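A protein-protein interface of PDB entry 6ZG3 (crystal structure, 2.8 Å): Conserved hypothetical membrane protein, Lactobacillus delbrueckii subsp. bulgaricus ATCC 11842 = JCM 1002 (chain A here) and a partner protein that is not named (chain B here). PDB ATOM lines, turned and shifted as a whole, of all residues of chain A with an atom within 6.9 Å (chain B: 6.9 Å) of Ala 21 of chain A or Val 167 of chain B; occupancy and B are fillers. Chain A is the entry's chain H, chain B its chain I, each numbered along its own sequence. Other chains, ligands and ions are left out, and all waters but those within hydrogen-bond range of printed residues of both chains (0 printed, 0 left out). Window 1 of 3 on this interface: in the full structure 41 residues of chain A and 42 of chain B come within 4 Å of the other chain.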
ATOM      1  N   VAL A  15      14.079 -27.243 -32.595  1.00  0.00           N
ATOM      2  CA  VAL A  15      15.409 -27.739 -32.245  1.00  0.00           C
ATOM      3  C   VAL A  15      16.058 -26.828 -31.203  1.00  0.00           C
ATOM      4  O   VAL A  15      16.624 -27.294 -30.198  1.00  0.00           O
ATOM      5  CB  VAL A  15      16.275 -27.841 -33.517  1.00  0.00           C
ATOM      6  CG1 VAL A  15      17.694 -28.162 -33.151  1.00  0.00           C
ATOM      7  CG2 VAL A  15      15.714 -28.881 -34.484  1.00  0.00           C
ATOM      8  N   SER A  16      15.939 -25.507 -31.410  1.00  0.00           N
ATOM      9  CA  SER A  16      16.381 -24.535 -30.420  1.00  0.00           C
ATOM     10  C   SER A  16      15.714 -24.772 -29.077  1.00  0.00           C
ATOM     11  O   SER A  16      16.368 -24.758 -28.037  1.00  0.00           O
ATOM     12  CB  SER A  16      16.064 -23.130 -30.909  1.00  0.00           C
ATOM     13  OG  SER A  16      16.773 -22.874 -32.098  1.00  0.00           O
ATOM     14  N   ALA A  17      14.398 -24.963 -29.076  1.00  0.00           N
ATOM     15  CA  ALA A  17      13.698 -25.096 -27.803  1.00  0.00           C
ATOM     16  C   ALA A  17      14.165 -26.325 -27.037  1.00  0.00           C
ATOM     17  O   ALA A  17      14.349 -26.280 -25.810  1.00  0.00           O
ATOM     18  CB  ALA A  17      12.197 -25.151 -28.051  1.00  0.00           C
ATOM     19  N   VAL A  18      14.372 -27.433 -27.747  1.00  0.00           N
ATOM     20  CA  VAL A  18      14.708 -28.666 -27.049  1.00  0.00           C
ATOM     21  C   VAL A  18      16.131 -28.600 -26.577  1.00  0.00           C
ATOM     22  O   VAL A  18      16.455 -29.111 -25.496  1.00  0.00           O
ATOM     23  CB  VAL A  18      14.469 -29.903 -27.929  1.00  0.00           C
ATOM     24  CG1 VAL A  18      12.956 -30.104 -28.133  1.00  0.00           C
ATOM     25  CG2 VAL A  18      15.235 -29.778 -29.255  1.00  0.00           C
ATOM     26  N   PHE A  19      16.999 -27.919 -27.349  1.00  0.00           N
ATOM     27  CA  PHE A  19      18.361 -27.690 -26.888  1.00  0.00           C
ATOM     28  C   PHE A  19      18.417 -26.707 -25.713  1.00  0.00           C
ATOM     29  O   PHE A  19      19.225 -26.906 -24.804  1.00  0.00           O
ATOM     30  CB  PHE A  19      19.239 -27.236 -28.052  1.00  0.00           C
ATOM     31  CG  PHE A  19      19.826 -28.381 -28.853  1.00  0.00           C
ATOM     32  CD1 PHE A  19      20.623 -29.342 -28.240  1.00  0.00           C
ATOM     33  CD2 PHE A  19      19.637 -28.462 -30.220  1.00  0.00           C
ATOM     34  CE1 PHE A  19      21.174 -30.374 -28.966  1.00  0.00           C
ATOM     35  CE2 PHE A  19      20.205 -29.494 -30.958  1.00  0.00           C
ATOM     36  CZ  PHE A  19      20.962 -30.447 -30.332  1.00  0.00           C
ATOM     37  N   VAL A  20      17.550 -25.680 -25.668  1.00  0.00           N
ATOM     38  CA  VAL A  20      17.515 -24.837 -24.471  1.00  0.00           C
ATOM     39  C   VAL A  20      17.040 -25.659 -23.287  1.00  0.00           C
ATOM     40  O   VAL A  20      17.570 -25.529 -22.178  1.00  0.00           O
ATOM     41  CB  VAL A  20      16.624 -23.583 -24.635  1.00  0.00           C
ATOM     42  CG1 VAL A  20      16.447 -22.866 -23.275  1.00  0.00           C
ATOM     43  CG2 VAL A  20      17.173 -22.629 -25.645  1.00  0.00           C
ATOM     44  N   ALA A  21      16.053 -26.536 -23.505  1.00  0.00           N
ATOM     45  CA  ALA A  21      15.570 -27.351 -22.401  1.00  0.00           C
ATOM     46  C   ALA A  21      16.684 -28.261 -21.874  1.00  0.00           C
ATOM     47  O   ALA A  21      16.892 -28.365 -20.657  1.00  0.00           O
ATOM     48  CB  ALA A  21      14.328 -28.148 -22.832  1.00  0.00           C
ATOM     49  N   ILE A  22      17.462 -28.867 -22.773  1.00  0.00           N
ATOM     50  CA  ILE A  22      18.594 -29.686 -22.334  1.00  0.00           C
ATOM     51  C   ILE A  22      19.635 -28.821 -21.614  1.00  0.00           C
ATOM     52  O   ILE A  22      20.238 -29.249 -20.620  1.00  0.00           O
ATOM     53  CB  ILE A  22      19.203 -30.442 -23.538  1.00  0.00           C
ATOM     54  CG1 ILE A  22      18.318 -31.638 -23.915  1.00  0.00           C
ATOM     55  CG2 ILE A  22      20.709 -30.822 -23.296  1.00  0.00           C
ATOM     56  CD1 ILE A  22      18.573 -32.168 -25.307  1.00  0.00           C
ATOM     57  N   LEU A  23      19.882 -27.601 -22.117  1.00  0.00           N
ATOM     58  CA  LEU A  23      20.886 -26.731 -21.509  1.00  0.00           C
ATOM     59  C   LEU A  23      20.492 -26.320 -20.102  1.00  0.00           C
ATOM     60  O   LEU A  23      21.340 -26.291 -19.198  1.00  0.00           O
ATOM     61  CB  LEU A  23      21.122 -25.505 -22.394  1.00  0.00           C
ATOM     62  CG  LEU A  23      21.971 -24.360 -21.839  1.00  0.00           C
ATOM     63  CD1 LEU A  23      23.233 -24.871 -21.179  1.00  0.00           C
ATOM     64  CD2 LEU A  23      22.302 -23.387 -22.957  1.00  0.00           C
ATOM     65  N   LEU A  24      19.213 -25.977 -19.907  1.00  0.00           N
ATOM     66  CA  LEU A  24      18.708 -25.677 -18.571  1.00  0.00           C
ATOM     67  C   LEU A  24      18.820 -26.898 -17.677  1.00  0.00           C
ATOM     68  O   LEU A  24      19.175 -26.780 -16.503  1.00  0.00           O
ATOM     69  CB  LEU A  24      17.264 -25.185 -18.645  1.00  0.00           C
ATOM     70  CG  LEU A  24      17.158 -23.886 -19.461  1.00  0.00           C
ATOM     71  CD1 LEU A  24      15.720 -23.445 -19.783  1.00  0.00           C
ATOM     72  CD2 LEU A  24      17.911 -22.779 -18.766  1.00  0.00           C
ATOM     73  N   LEU A  25      18.524 -28.083 -18.218  1.00  0.00           N
ATOM     74  CA  LEU A  25      18.657 -29.294 -17.422  1.00  0.00           C
ATOM     75  C   LEU A  25      20.096 -29.496 -16.988  1.00  0.00           C
ATOM     76  O   LEU A  25      20.360 -29.820 -15.828  1.00  0.00           O
ATOM     77  CB  LEU A  25      18.125 -30.510 -18.193  1.00  0.00           C
ATOM     78  CG  LEU A  25      16.610 -30.801 -18.097  1.00  0.00           C
ATOM     79  CD1 LEU A  25      16.217 -32.023 -18.884  1.00  0.00           C
ATOM     80  CD2 LEU A  25      16.195 -31.005 -16.669  1.00  0.00           C
ATOM     81  N   GLU A  26      21.043 -29.292 -17.901  1.00  0.00           N
ATOM     82  CA  GLU A  26      22.443 -29.527 -17.559  1.00  0.00           C
ATOM     83  C   GLU A  26      22.941 -28.487 -16.560  1.00  0.00           C
ATOM     84  O   GLU A  26      23.672 -28.822 -15.621  1.00  0.00           O
ATOM     85  CB  GLU A  26      23.310 -29.503 -18.817  1.00  0.00           C
ATOM     86  CG  GLU A  26      22.924 -30.555 -19.821  1.00  0.00           C
ATOM     87  CD  GLU A  26      23.881 -30.640 -20.979  1.00  0.00           C
ATOM     88  OE1 GLU A  26      23.929 -29.704 -21.799  1.00  0.00           O
ATOM     89  OE2 GLU A  26      24.584 -31.672 -21.074  1.00  0.00           O
ATOM     90  N   ILE A  29      20.381 -28.572 -13.070  1.00  0.00           N
ATOM     91  CA  ILE A  29      20.340 -29.907 -12.460  1.00  0.00           C
ATOM     92  C   ILE A  29      21.757 -30.460 -12.398  1.00  0.00           C
ATOM     93  O   ILE A  29      22.549 -30.257 -13.335  1.00  0.00           O
ATOM     94  CB  ILE A  29      19.424 -30.879 -13.224  1.00  0.00           C
ATOM     95  CG1 ILE A  29      18.032 -30.296 -13.426  1.00  0.00           C
ATOM     96  CG2 ILE A  29      19.315 -32.178 -12.495  1.00  0.00           C
ATOM     97  CD1 ILE A  29      17.301 -29.977 -12.127  1.00  0.00           C
ATOM     98  N   PHE A  66      23.508 -19.895 -29.400  1.00  0.00           N
ATOM     99  CA  PHE A  66      23.381 -20.873 -28.327  1.00  0.00           C
ATOM    100  C   PHE A  66      24.460 -20.647 -27.280  1.00  0.00           C
ATOM    101  O   PHE A  66      24.214 -20.802 -26.080  1.00  0.00           O
ATOM    102  CB  PHE A  66      23.490 -22.297 -28.868  1.00  0.00           C
ATOM    103  CG  PHE A  66      22.928 -23.367 -27.941  1.00  0.00           C
ATOM    104  CD1 PHE A  66      21.604 -23.328 -27.521  1.00  0.00           C
ATOM    105  CD2 PHE A  66      23.723 -24.405 -27.473  1.00  0.00           C
ATOM    106  CE1 PHE A  66      21.076 -24.328 -26.673  1.00  0.00           C
ATOM    107  CE2 PHE A  66      23.196 -25.387 -26.619  1.00  0.00           C
ATOM    108  CZ  PHE A  66      21.880 -25.337 -26.219  1.00  0.00           C
ATOM    109  N   ILE B   6      10.203 -25.888 -14.090  1.00  0.00           N
ATOM    110  CA  ILE B   6       9.293 -25.786 -12.954  1.00  0.00           C
ATOM    111  C   ILE B   6      10.087 -25.425 -11.694  1.00  0.00           C
ATOM    112  O   ILE B   6      10.629 -26.300 -11.011  1.00  0.00           O
ATOM    113  CB  ILE B   6       8.471 -27.092 -12.772  1.00  0.00           C
ATOM    114  CG1 ILE B   6       7.520 -27.280 -13.946  1.00  0.00           C
ATOM    115  CG2 ILE B   6       7.639 -27.057 -11.506  1.00  0.00           C
ATOM    116  CD1 ILE B   6       6.632 -28.484 -13.790  1.00  0.00           C
ATOM    117  N   VAL B 159      10.557 -20.036 -28.086  1.00  0.00           N
ATOM    118  CA  VAL B 159      11.601 -20.973 -27.683  1.00  0.00           C
ATOM    119  C   VAL B 159      11.606 -21.114 -26.168  1.00  0.00           C
ATOM    120  O   VAL B 159      11.604 -22.226 -25.628  1.00  0.00           O
ATOM    121  CB  VAL B 159      12.977 -20.523 -28.231  1.00  0.00           C
ATOM    122  CG1 VAL B 159      14.078 -21.472 -27.804  1.00  0.00           C
ATOM    123  CG2 VAL B 159      12.964 -20.489 -29.738  1.00  0.00           C
ATOM    124  N   ILE B 162       8.366 -23.229 -25.047  1.00  0.00           N
ATOM    125  CA  ILE B 162       8.467 -24.646 -25.376  1.00  0.00           C
ATOM    126  C   ILE B 162       9.513 -25.323 -24.501  1.00  0.00           C
ATOM    127  O   ILE B 162       9.257 -26.374 -23.892  1.00  0.00           O
ATOM    128  CB  ILE B 162       8.751 -24.823 -26.882  1.00  0.00           C
ATOM    129  CG1 ILE B 162       7.553 -24.302 -27.679  1.00  0.00           C
ATOM    130  CG2 ILE B 162       9.019 -26.271 -27.223  1.00  0.00           C
ATOM    131  CD1 ILE B 162       7.822 -24.026 -29.111  1.00  0.00           C
ATOM    132  N   ALA B 163      10.697 -24.719 -24.413  1.00  0.00           N
ATOM    133  CA  ALA B 163      11.761 -25.262 -23.587  1.00  0.00           C
ATOM    134  C   ALA B 163      11.284 -25.487 -22.163  1.00  0.00           C
ATOM    135  O   ALA B 163      11.463 -26.571 -21.599  1.00  0.00           O
ATOM    136  CB  ALA B 163      12.972 -24.321 -23.619  1.00  0.00           C
ATOM    137  N   LEU B 164      10.711 -24.458 -21.548  1.00  0.00           N
ATOM    138  CA  LEU B 164      10.290 -24.605 -20.164  1.00  0.00           C
ATOM    139  C   LEU B 164       9.204 -25.668 -20.030  1.00  0.00           C
ATOM    140  O   LEU B 164       9.061 -26.272 -18.952  1.00  0.00           O
ATOM    141  CB  LEU B 164       9.792 -23.256 -19.625  1.00  0.00           C
ATOM    142  CG  LEU B 164      10.867 -22.198 -19.403  1.00  0.00           C
ATOM    143  CD1 LEU B 164      10.202 -20.870 -19.125  1.00  0.00           C
ATOM    144  CD2 LEU B 164      11.806 -22.607 -18.249  1.00  0.00           C
ATOM    145  N   ARG B 165       8.448 -25.902 -21.111  1.00  0.00           N
ATOM    146  CA  ARG B 165       7.352 -26.857 -21.091  1.00  0.00           C
ATOM    147  C   ARG B 165       7.855 -28.299 -21.161  1.00  0.00           C
ATOM    148  O   ARG B 165       7.254 -29.207 -20.560  1.00  0.00           O
ATOM    149  CB  ARG B 165       6.428 -26.538 -22.272  1.00  0.00           C
ATOM    150  CG  ARG B 165       5.313 -27.535 -22.538  1.00  0.00           C
ATOM    151  CD  ARG B 165       5.633 -28.521 -23.623  1.00  0.00           C
ATOM    152  NE  ARG B 165       5.758 -29.828 -22.999  1.00  0.00           N
ATOM    153  CZ  ARG B 165       5.481 -30.962 -23.612  1.00  0.00           C
ATOM    154  NH1 ARG B 165       5.071 -30.944 -24.878  1.00  0.00           N
ATOM    155  NH2 ARG B 165       5.614 -32.112 -22.960  1.00  0.00           N
ATOM    156  N   PHE B 166       8.962 -28.509 -21.881  1.00  0.00           N
ATOM    157  CA  PHE B 166       9.625 -29.806 -22.032  1.00  0.00           C
ATOM    158  C   PHE B 166      10.703 -30.088 -20.982  1.00  0.00           C
ATOM    159  O   PHE B 166      11.212 -31.214 -20.928  1.00  0.00           O
ATOM    160  CB  PHE B 166      10.284 -29.893 -23.404  1.00  0.00           C
ATOM    161  CG  PHE B 166       9.396 -30.411 -24.478  1.00  0.00           C
ATOM    162  CD1 PHE B 166       9.175 -31.784 -24.614  1.00  0.00           C
ATOM    163  CD2 PHE B 166       8.780 -29.525 -25.367  1.00  0.00           C
ATOM    164  CE1 PHE B 166       8.359 -32.274 -25.624  1.00  0.00           C
ATOM    165  CE2 PHE B 166       7.970 -29.997 -26.390  1.00  0.00           C
ATOM    166  CZ  PHE B 166       7.752 -31.374 -26.518  1.00  0.00           C
ATOM    167  N   VAL B 167      11.113 -29.093 -20.205  1.00  0.00           N
ATOM    168  CA  VAL B 167      12.154 -29.308 -19.200  1.00  0.00           C
ATOM    169  C   VAL B 167      11.746 -30.457 -18.271  1.00  0.00           C
ATOM    170  O   VAL B 167      12.576 -31.315 -17.956  1.00  0.00           O
ATOM    171  CB  VAL B 167      12.489 -27.995 -18.450  1.00  0.00           C
ATOM    172  CG1 VAL B 167      13.022 -28.249 -17.051  1.00  0.00           C
ATOM    173  CG2 VAL B 167      13.507 -27.219 -19.243  1.00  0.00           C
ATOM    174  N   PRO B 168      10.522 -30.564 -17.833  1.00  0.00           N
ATOM    175  CA  PRO B 168      10.215 -31.684 -16.931  1.00  0.00           C
ATOM    176  C   PRO B 168       9.971 -32.994 -17.690  1.00  0.00           C
ATOM    177  O   PRO B 168      10.251 -34.091 -17.189  1.00  0.00           O
ATOM    178  CB  PRO B 168       8.977 -31.189 -16.189  1.00  0.00           C
ATOM    179  CG  PRO B 168       8.329 -30.247 -17.166  1.00  0.00           C
ATOM    180  CD  PRO B 168       9.350 -29.693 -18.057  1.00  0.00           C
ATOM    181  N   THR B 169       9.458 -32.872 -18.919  1.00  0.00           N
ATOM    182  CA  THR B 169       9.256 -34.043 -19.766  1.00  0.00           C
ATOM    183  C   THR B 169      10.596 -34.697 -20.115  1.00  0.00           C
ATOM    184  O   THR B 169      10.783 -35.911 -19.909  1.00  0.00           O
ATOM    185  CB  THR B 169       8.466 -33.642 -21.038  1.00  0.00           C
ATOM    186  OG1 THR B 169       7.044 -33.678 -20.795  1.00  0.00           O
ATOM    187  CG2 THR B 169       8.783 -34.550 -22.212  1.00  0.00           C
ATOM    188  N   LEU B 170      11.572 -33.890 -20.577  1.00  0.00           N
ATOM    189  CA  LEU B 170      12.877 -34.450 -20.902  1.00  0.00           C
ATOM    190  C   LEU B 170      13.591 -34.924 -19.662  1.00  0.00           C
ATOM    191  O   LEU B 170      14.420 -35.827 -19.745  1.00  0.00           O
ATOM    192  CB  LEU B 170      13.752 -33.470 -21.666  1.00  0.00           C
ATOM    193  CG  LEU B 170      13.303 -33.226 -23.098  1.00  0.00           C
ATOM    194  CD1 LEU B 170      14.225 -32.252 -23.859  1.00  0.00           C
ATOM    195  CD2 LEU B 170      13.210 -34.524 -23.816  1.00  0.00           C
ATOM    196  N   PHE B 171      13.268 -34.359 -18.505  1.00  0.00           N
ATOM    197  CA  PHE B 171      13.880 -34.847 -17.275  1.00  0.00           C
ATOM    198  C   PHE B 171      13.384 -36.231 -16.937  1.00  0.00           C
ATOM    199  O   PHE B 171      14.175 -37.112 -16.575  1.00  0.00           O
ATOM    200  CB  PHE B 171      13.576 -33.891 -16.127  1.00  0.00           C
ATOM    201  CG  PHE B 171      14.054 -34.360 -14.781  1.00  0.00           C
ATOM    202  CD1 PHE B 171      15.293 -33.996 -14.310  1.00  0.00           C
ATOM    203  CD2 PHE B 171      13.231 -35.104 -13.966  1.00  0.00           C
ATOM    204  CE1 PHE B 171      15.707 -34.394 -13.064  1.00  0.00           C
ATOM    205  CE2 PHE B 171      13.642 -35.499 -12.728  1.00  0.00           C
ATOM    206  CZ  PHE B 171      14.881 -35.144 -12.274  1.00  0.00           C
ATOM    207  N   ASP B 172      12.081 -36.458 -17.065  1.00  0.00           N
ATOM    208  CA  ASP B 172      11.589 -37.800 -16.800  1.00  0.00           C
ATOM    209  C   ASP B 172      12.198 -38.783 -17.781  1.00  0.00           C
ATOM    210  O   ASP B 172      12.697 -39.840 -17.375  1.00  0.00           O
ATOM    211  CB  ASP B 172      10.067 -37.853 -16.843  1.00  0.00           C
ATOM    212  CG  ASP B 172       9.422 -36.987 -15.766  1.00  0.00           C
ATOM    213  OD1 ASP B 172      10.090 -36.059 -15.240  1.00  0.00           O
ATOM    214  OD2 ASP B 172       8.247 -37.252 -15.427  1.00  0.00           O
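C of Ser 16 of chain A touches CG1 of Val 159 of chain B, at 3.9 Å.
CA of Ala 17 of chain A touches CG1 of Val 159 of chain B, 3.6 Å away.
Ala 17 of chain A touches Ala 163 of chain B (O to CB, 3.2 Å).
Val 159 of chain B touches Val 20 of chain A (CG1 to CG2, 3.9 Å).
Val 20 of chain A touches Ala 163 of chain B (CG1 to CB, 3.8 Å).
Ala 21 of chain A touches Ala 163 of chain B.
CG2 of Val 167 of chain B touches CA of Ala 21 of chain A (3.8 Å).
Leu 25 of chain A touches Val 167 of chain B (CD1 to O, 3.8 Å).
Leu 25 of chain A touches Leu 170 of chain B (CD1 to CB, 3.99 Å).
Leu 25 of chain A touches Phe 171 of chain B (CD1 to N, 3.8 Å).
Of the printed residues of chain B, Ser 16 of chain A touches Val 159.
Printed residues of chain B within 4 Å of Ala 21 of chain A: Ala 163 and Val 167.
Of the printed residues of chain A, Ala 163 of chain B touches Ala 17, Val 20 and Ala 21.
Of chain A, only Ala 21 (3.8 Å) and Leu 25 (3.8 Å) come within 4 Å of Val 167 of chain B.
The nearest printed residue of chain A that does not touch Ala 163 of chain B is Leu 24 of chain A (4.8 Å).
Of the 13 printed residues of chain B, 6 touch a printed residue of chain A.
Printed residues of chain B that touch a printed residue of chain A: Val 159, Ile 162, Ala 163, Val 167, Leu 170 and Phe 171.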
